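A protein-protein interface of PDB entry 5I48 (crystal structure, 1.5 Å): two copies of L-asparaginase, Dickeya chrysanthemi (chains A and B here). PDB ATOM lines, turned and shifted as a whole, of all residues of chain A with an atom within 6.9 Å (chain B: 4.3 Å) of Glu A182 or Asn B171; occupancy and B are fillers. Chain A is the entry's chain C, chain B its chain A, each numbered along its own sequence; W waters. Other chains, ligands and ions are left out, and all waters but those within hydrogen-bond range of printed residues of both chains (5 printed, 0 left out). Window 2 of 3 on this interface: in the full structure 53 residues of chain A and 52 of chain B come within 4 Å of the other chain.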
ATOM      1  N   LYS A 179     -18.644  -9.752  14.143  1.00  0.00           N
ATOM      2  CA  LYS A 179     -19.643  -8.996  13.382  1.00  0.00           C
ATOM      3  C   LYS A 179     -18.929  -7.920  12.514  1.00  0.00           C
ATOM      4  O   LYS A 179     -17.789  -7.544  12.806  1.00  0.00           O
ATOM      5  CB  LYS A 179     -20.581  -8.225  14.318  1.00  0.00           C
ATOM      6  CG  LYS A 179     -21.241  -9.058  15.376  1.00  0.00           C
ATOM      7  CD  LYS A 179     -22.114  -8.250  16.284  1.00  0.00           C
ATOM      8  CE  LYS A 179     -22.552  -8.993  17.508  1.00  0.00           C
ATOM      9  NZ  LYS A 179     -23.446 -10.115  17.274  1.00  0.00           N
ATOM     10  N   ALA A 180     -19.606  -7.473  11.494  1.00  0.00           N
ATOM     11  CA  ALA A 180     -19.147  -6.332  10.718  1.00  0.00           C
ATOM     12  C   ALA A 180     -20.381  -5.407  10.663  1.00  0.00           C
ATOM     13  O   ALA A 180     -21.250  -5.520   9.845  1.00  0.00           O
ATOM     14  CB  ALA A 180     -18.739  -6.818   9.345  1.00  0.00           C
ATOM     15  N   ASN A 181     -20.456  -4.496  11.635  1.00  0.00           N
ATOM     16  CA  ASN A 181     -21.703  -3.789  11.824  1.00  0.00           C
ATOM     17  C   ASN A 181     -22.180  -3.084  10.573  1.00  0.00           C
ATOM     18  O   ASN A 181     -23.374  -3.111  10.243  1.00  0.00           O
ATOM     19  CB  ASN A 181     -21.622  -2.827  13.001  1.00  0.00           C
ATOM     20  CG  ASN A 181     -21.453  -3.575  14.328  1.00  0.00           C
ATOM     21  OD1 ASN A 181     -22.232  -4.494  14.661  1.00  0.00           O
ATOM     22  ND2 ASN A 181     -20.383  -3.255  15.038  1.00  0.00           N
ATOM     23  N   GLU A 182     -21.270  -2.410   9.905  1.00  0.00           N
ATOM     24  CA  GLU A 182     -21.691  -1.603   8.742  1.00  0.00           C
ATOM     25  C   GLU A 182     -21.698  -2.364   7.409  1.00  0.00           C
ATOM     26  O   GLU A 182     -22.288  -1.930   6.484  1.00  0.00           O
ATOM     27  CB  GLU A 182     -20.753  -0.380   8.613  1.00  0.00           C
ATOM     28  CG  GLU A 182     -20.958   0.611   9.822  1.00  0.00           C
ATOM     29  CD  GLU A 182     -22.213   1.407   9.730  1.00  0.00           C
ATOM     30  OE1 GLU A 182     -22.411   2.067   8.694  1.00  0.00           O
ATOM     31  OE2 GLU A 182     -22.980   1.431  10.751  1.00  0.00           O
ATOM     32  N   GLU A 183     -20.927  -3.409   7.349  1.00  0.00           N
ATOM     33  CA  GLU A 183     -20.722  -4.162   6.089  1.00  0.00           C
ATOM     34  C   GLU A 183     -21.364  -5.523   6.037  1.00  0.00           C
ATOM     35  O   GLU A 183     -21.487  -6.101   4.951  1.00  0.00           O
ATOM     36  CB  GLU A 183     -19.235  -4.377   5.832  1.00  0.00           C
ATOM     37  CG  GLU A 183     -18.423  -3.093   5.869  1.00  0.00           C
ATOM     38  CD  GLU A 183     -17.787  -2.774   7.176  1.00  0.00           C
ATOM     39  OE1 GLU A 183     -18.145  -3.391   8.230  1.00  0.00           O
ATOM     40  OE2 GLU A 183     -16.958  -1.806   7.201  1.00  0.00           O
ATOM     41  N   GLY A 184     -21.840  -6.008   7.172  1.00  0.00           N
ATOM     42  CA  GLY A 184     -22.516  -7.288   7.215  1.00  0.00           C
ATOM     43  C   GLY A 184     -21.625  -8.461   6.904  1.00  0.00           C
ATOM     44  O   GLY A 184     -20.437  -8.374   6.814  1.00  0.00           O
ATOM     45  N   GLY A 252     -12.731   9.487  18.077  1.00  0.00           N
ATOM     46  CA  GLY A 252     -13.592   9.797  16.949  1.00  0.00           C
ATOM     47  C   GLY A 252     -12.990   9.454  15.592  1.00  0.00           C
ATOM     48  O   GLY A 252     -12.414   8.339  15.408  1.00  0.00           O
ATOM     49  N   ALA A 253     -13.104  10.417  14.660  1.00  0.00           N
ATOM     50  CA  ALA A 253     -12.644  10.207  13.309  1.00  0.00           C
ATOM     51  C   ALA A 253     -11.173  10.534  13.184  1.00  0.00           C
ATOM     52  O   ALA A 253     -10.788  11.413  12.462  1.00  0.00           O
ATOM     53  CB  ALA A 253     -13.494  11.019  12.368  1.00  0.00           C
ATOM     54  N   THR A 278      -9.321   4.766  14.102  1.00  0.00           N
ATOM     55  CA  THR A 278     -10.309   5.133  15.165  1.00  0.00           C
ATOM     56  C   THR A 278     -10.395   4.092  16.203  1.00  0.00           C
ATOM     57  O   THR A 278     -10.342   2.889  15.909  1.00  0.00           O
ATOM     58  CB  THR A 278     -11.693   5.420  14.536  1.00  0.00           C
ATOM     59  OG1 THR A 278     -12.614   5.763  15.542  1.00  0.00           O
ATOM     60  CG2 THR A 278     -12.240   4.243  13.735  1.00  0.00           C
ATOM     61  N   THR A 280     -13.116   3.803  17.860  1.00  0.00           N
ATOM     62  CA  THR A 280     -14.580   3.684  18.058  1.00  0.00           C
ATOM     63  C   THR A 280     -15.118   2.292  17.776  1.00  0.00           C
ATOM     64  O   THR A 280     -16.070   1.861  18.440  1.00  0.00           O
ATOM     65  CB  THR A 280     -15.380   4.686  17.226  1.00  0.00           C
ATOM     66  OG1 THR A 280     -15.131   4.485  15.854  1.00  0.00           O
ATOM     67  CG2 THR A 280     -15.046   6.088  17.613  1.00  0.00           C
ATOM     68  N   GLY A 281     -14.559   1.616  16.803  1.00  0.00           N
ATOM     69  CA  GLY A 281     -14.999   0.303  16.441  1.00  0.00           C
ATOM     70  C   GLY A 281     -15.474   0.160  15.012  1.00  0.00           C
ATOM     71  O   GLY A 281     -15.430  -0.942  14.429  1.00  0.00           O
ATOM     72  N   ASN A 282     -15.884   1.244  14.395  1.00  0.00           N
ATOM     73  CA  ASN A 282     -16.518   1.206  13.092  1.00  0.00           C
ATOM     74  C   ASN A 282     -16.359   2.524  12.361  1.00  0.00           C
ATOM     75  O   ASN A 282     -16.213   3.568  12.975  1.00  0.00           O
ATOM     76  CB  ASN A 282     -18.048   0.978  13.224  1.00  0.00           C
ATOM     77  CG  ASN A 282     -18.461  -0.277  14.039  1.00  0.00           C
ATOM     78  OD1 ASN A 282     -18.660  -1.312  13.510  1.00  0.00           O
ATOM     79  ND2 ASN A 282     -18.503  -0.124  15.384  1.00  0.00           N
ATOM     80  N   GLY A 283     -16.547   2.499  11.059  1.00  0.00           N
ATOM     81  CA  GLY A 283     -16.743   3.697  10.290  1.00  0.00           C
ATOM     82  C   GLY A 283     -15.525   4.269   9.606  1.00  0.00           C
ATOM     83  O   GLY A 283     -14.437   3.734   9.687  1.00  0.00           O
ATOM     84  N   ILE A 284     -15.751   5.390   8.931  1.00  0.00           N
ATOM     85  CA  ILE A 284     -14.746   6.005   8.056  1.00  0.00           C
ATOM     86  C   ILE A 284     -13.992   7.130   8.762  1.00  0.00           C
ATOM     87  O   ILE A 284     -14.600   8.038   9.332  1.00  0.00           O
ATOM     88  CB  ILE A 284     -15.450   6.661   6.877  1.00  0.00           C
ATOM     89  CG1 ILE A 284     -16.252   5.676   6.040  1.00  0.00           C
ATOM     90  CG2 ILE A 284     -14.490   7.462   6.016  1.00  0.00           C
ATOM     91  CD1 ILE A 284     -15.380   4.712   5.312  1.00  0.00           C
ATOM     92  N   LYS B 169     -18.933   6.200  21.732  1.00  0.00           N
ATOM     93  CA  LYS B 169     -18.953   6.555  20.369  1.00  0.00           C
ATOM     94  C   LYS B 169     -18.466   5.320  19.577  1.00  0.00           C
ATOM     95  O   LYS B 169     -17.304   4.898  19.718  1.00  0.00           O
ATOM     96  CB  LYS B 169     -18.065   7.724  20.081  1.00  0.00           C
ATOM     97  CG  LYS B 169     -18.146   8.293  18.685  1.00  0.00           C
ATOM     98  CD  LYS B 169     -17.355   9.610  18.500  1.00  0.00           C
ATOM     99  CE  LYS B 169     -17.450  10.116  17.097  1.00  0.00           C
ATOM    100  NZ  LYS B 169     -16.876  11.440  16.882  1.00  0.00           N
ATOM    101  N   THR B 170     -19.371   4.684  18.829  1.00  0.00           N
ATOM    102  CA  THR B 170     -19.061   3.404  18.161  1.00  0.00           C
ATOM    103  C   THR B 170     -18.662   3.572  16.729  1.00  0.00           C
ATOM    104  O   THR B 170     -18.183   2.591  16.130  1.00  0.00           O
ATOM    105  CB  THR B 170     -20.234   2.417  18.221  1.00  0.00           C
ATOM    106  OG1 THR B 170     -21.323   2.852  17.383  1.00  0.00           O
ATOM    107  CG2 THR B 170     -20.749   2.156  19.605  1.00  0.00           C
ATOM    108  N   ASN B 171     -18.867   4.747  16.158  1.00  0.00           N
ATOM    109  CA  ASN B 171     -18.557   4.949  14.730  1.00  0.00           C
ATOM    110  C   ASN B 171     -17.890   6.307  14.626  1.00  0.00           C
ATOM    111  O   ASN B 171     -18.224   7.252  15.282  1.00  0.00           O
ATOM    112  CB  ASN B 171     -19.894   4.914  13.934  1.00  0.00           C
ATOM    113  CG  ASN B 171     -19.669   4.901  12.398  1.00  0.00           C
ATOM    114  OD1 ASN B 171     -19.131   5.864  11.840  1.00  0.00           O
ATOM    115  ND2 ASN B 171     -20.057   3.839  11.727  1.00  0.00           N
ATOM    116  N   ALA B 172     -16.862   6.352  13.773  1.00  0.00           N
ATOM    117  CA  ALA B 172     -16.093   7.573  13.581  1.00  0.00           C
ATOM    118  C   ALA B 172     -16.900   8.741  13.135  1.00  0.00           C
ATOM    119  O   ALA B 172     -16.612   9.851  13.537  1.00  0.00           O
ATOM    120  CB  ALA B 172     -15.032   7.298  12.535  1.00  0.00           C
ATOM    121  N   SER B 173     -17.947   8.502  12.345  1.00  0.00           N
ATOM    122  CA  SER B 173     -18.539   9.562  11.546  1.00  0.00           C
ATOM    123  C   SER B 173     -20.039   9.655  11.356  1.00  0.00           C
ATOM    124  O   SER B 173     -20.495  10.613  10.767  1.00  0.00           O
ATOM    125  CB  SER B 173     -17.862   9.530  10.198  1.00  0.00           C
ATOM    126  OG  SER B 173     -16.492   9.777  10.240  1.00  0.00           O
ATOM    127  N   THR B 174     -20.798   8.789  11.924  1.00  0.00           N
ATOM    128  CA  THR B 174     -22.264   8.789  11.719  1.00  0.00           C
ATOM    129  C   THR B 174     -23.078   9.478  12.834  1.00  0.00           C
ATOM    130  O   THR B 174     -22.648   9.589  13.959  1.00  0.00           O
ATOM    131  CB  THR B 174     -22.738   7.346  11.617  1.00  0.00           C
ATOM    132  OG1 THR B 174     -22.320   6.644  12.779  1.00  0.00           O
ATOM    133  CG2 THR B 174     -22.194   6.676  10.403  1.00  0.00           C
ATOM    134  N   THR B 177     -23.891   7.234  15.998  1.00  0.00           N
ATOM    135  CA  THR B 177     -22.728   6.618  16.566  1.00  0.00           C
ATOM    136  C   THR B 177     -22.817   6.242  18.034  1.00  0.00           C
ATOM    137  O   THR B 177     -22.247   5.210  18.417  1.00  0.00           O
ATOM    138  CB  THR B 177     -21.525   7.555  16.324  1.00  0.00           C
ATOM    139  OG1 THR B 177     -20.347   6.969  16.789  1.00  0.00           O
ATOM    140  CG2 THR B 177     -21.738   8.876  17.050  1.00  0.00           C
HETATM  141  O   HOH W   1     -21.814   1.927  13.146  1.00  0.00           O
HETATM  142  O   HOH W   2     -18.622   6.171   9.123  1.00  0.00           O
HETATM  143  O   HOH W   3     -16.484   2.429  21.327  1.00  0.00           O
HETATM  144  O   HOH W   4     -20.014   3.653   8.623  1.00  0.00           O
HETATM  145  O   HOH W   5     -21.883   0.749  15.611  1.00  0.00           O
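Printed residues of chain A that touch a printed residue of chain B: Glu A182, Gly A252, Ala A253, Thr A280, Gly A281, Asn A282, Gly A283 and Ile A284. Hydrophobic or aromatic side chains of chain A within 4 Å of the printed part of chain B: Ala A253. Along chain A the printed residues that touch a printed residue of chain B span positions 182 to 284. Of the 7 printed residues of chain B, 5 touch a printed residue of chain A. Printed residues of chain B that touch a printed residue of chain A: Lys B169, Thr B170, Asn B171, Ala B172 and Ser B173. Hydrophobic or aromatic side chains of chain B that line the printed part of chain A: Ala B172. Among the printed residues, 15 pairs touch across the chains.
Glu A182 touches Asn B171. Gly A252 touches Lys B169 (CA to NZ, 3.7 Å). O of Ala B172 touches CB of Ala A253 (3.5 Å). OG of Ser B173 touches CB of Ala A253, 3.9 Å away. Thr A280 touches Lys B169 (CB to O, 3.2 Å). C of Asn B171 touches OG1 of Thr A280 (3.5 Å). Thr B170 touches Gly A281. CA of Asn B171 touches O of Asn A282, 3.2 Å away. Gly A283 touches Asn B171. Ala B172 touches Ile A284 (CB to O, 3.3 Å).
Glu A182 touches one residue of chain B. Printed residues of chain B within 4 Å of Gly A281: Thr B170 (3.8 Å). Printed residues of chain B within 4 Å of Ala A253: Ala B172 (3.5 Å) and Ser B173 (3.9 Å). Of the printed residues of chain A, Lys B169 touches Gly A252 (3.7 Å) and Thr A280 (3.2 Å). Thr A278 touches none of the printed residues of chain B. Thr B174 touches none of the printed residues of chain A. The nearest printed residue of chain B that does not touch Glu A182 is Thr B174 (4.9 Å). The nearest residue of chain A that does not touch Asn B171 is Ile A284 (4.5 Å). The nearest printed residue of chain A that does not touch Ser B173 is Asn A282 (5.3 Å).
OG1 of Thr A280 is in hydrogen-bond range of N of Ala B172, at 3.3 Å. O of Asn A282 lies within hydrogen-bond range of N of Ala B172. O of Thr B170 is in hydrogen-bond range of ND2 of Asn A282, at 2.8 Å. OG of Ser B173 sits at hydrogen-bond distance from O of Ile A284. O of Thr B170 sits close to O of Thr A280.
Water W1 bridges OE2 of Glu A182 and ND2 of Asn B171. Water W2 bridges the side-chain amide oxygen (OD1) of Asn B171 (2.8 Å) and the backbone NH (N) of Ile A284 (3.0 Å). Water W5 lies within hydrogen-bond range of OG1 of Thr B170 (2.8 Å) and ND2 of Asn A282 (3.5 Å). Water W4 bridges OE1 of Glu A182 and ND2 of Asn B171. Water W3 bridges O of Thr A280 and O of Lys B169.
No position is printed for both chains. Of the 15 pairs that touch across the chains among the printed residues, none has its exchanged pair printed and touching as well.
The side-chain hydroxyl (OG1) of Thr A280 is in hydrogen-bond range of the backbone carbonyl oxygen (O) of Asn A282, 3.2 Å away. The side-chain amide oxygen (OD1) of Asn A282 sits at hydrogen-bond distance from the side-chain amide nitrogen (ND2) of Asn A181 (3.0 Å). The side-chain hydroxyl (OG1) of Thr B170 lies within hydrogen-bond range of the backbone carbonyl oxygen (O) of Thr B177, 2.7 Å away. The side-chain amide oxygen (OD1) of Asn B171 is in hydrogen-bond range of the backbone NH (N) of Thr B174. The side-chain amide oxygen (OD1) of Asn B171 is in hydrogen-bond range of the backbone NH (N) of Ser B173 (2.9 Å). The backbone carbonyl oxygen (O) of Asn B171 is in hydrogen-bond range of the side-chain hydroxyl (OG1) of Thr B177, at 2.6 Å.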
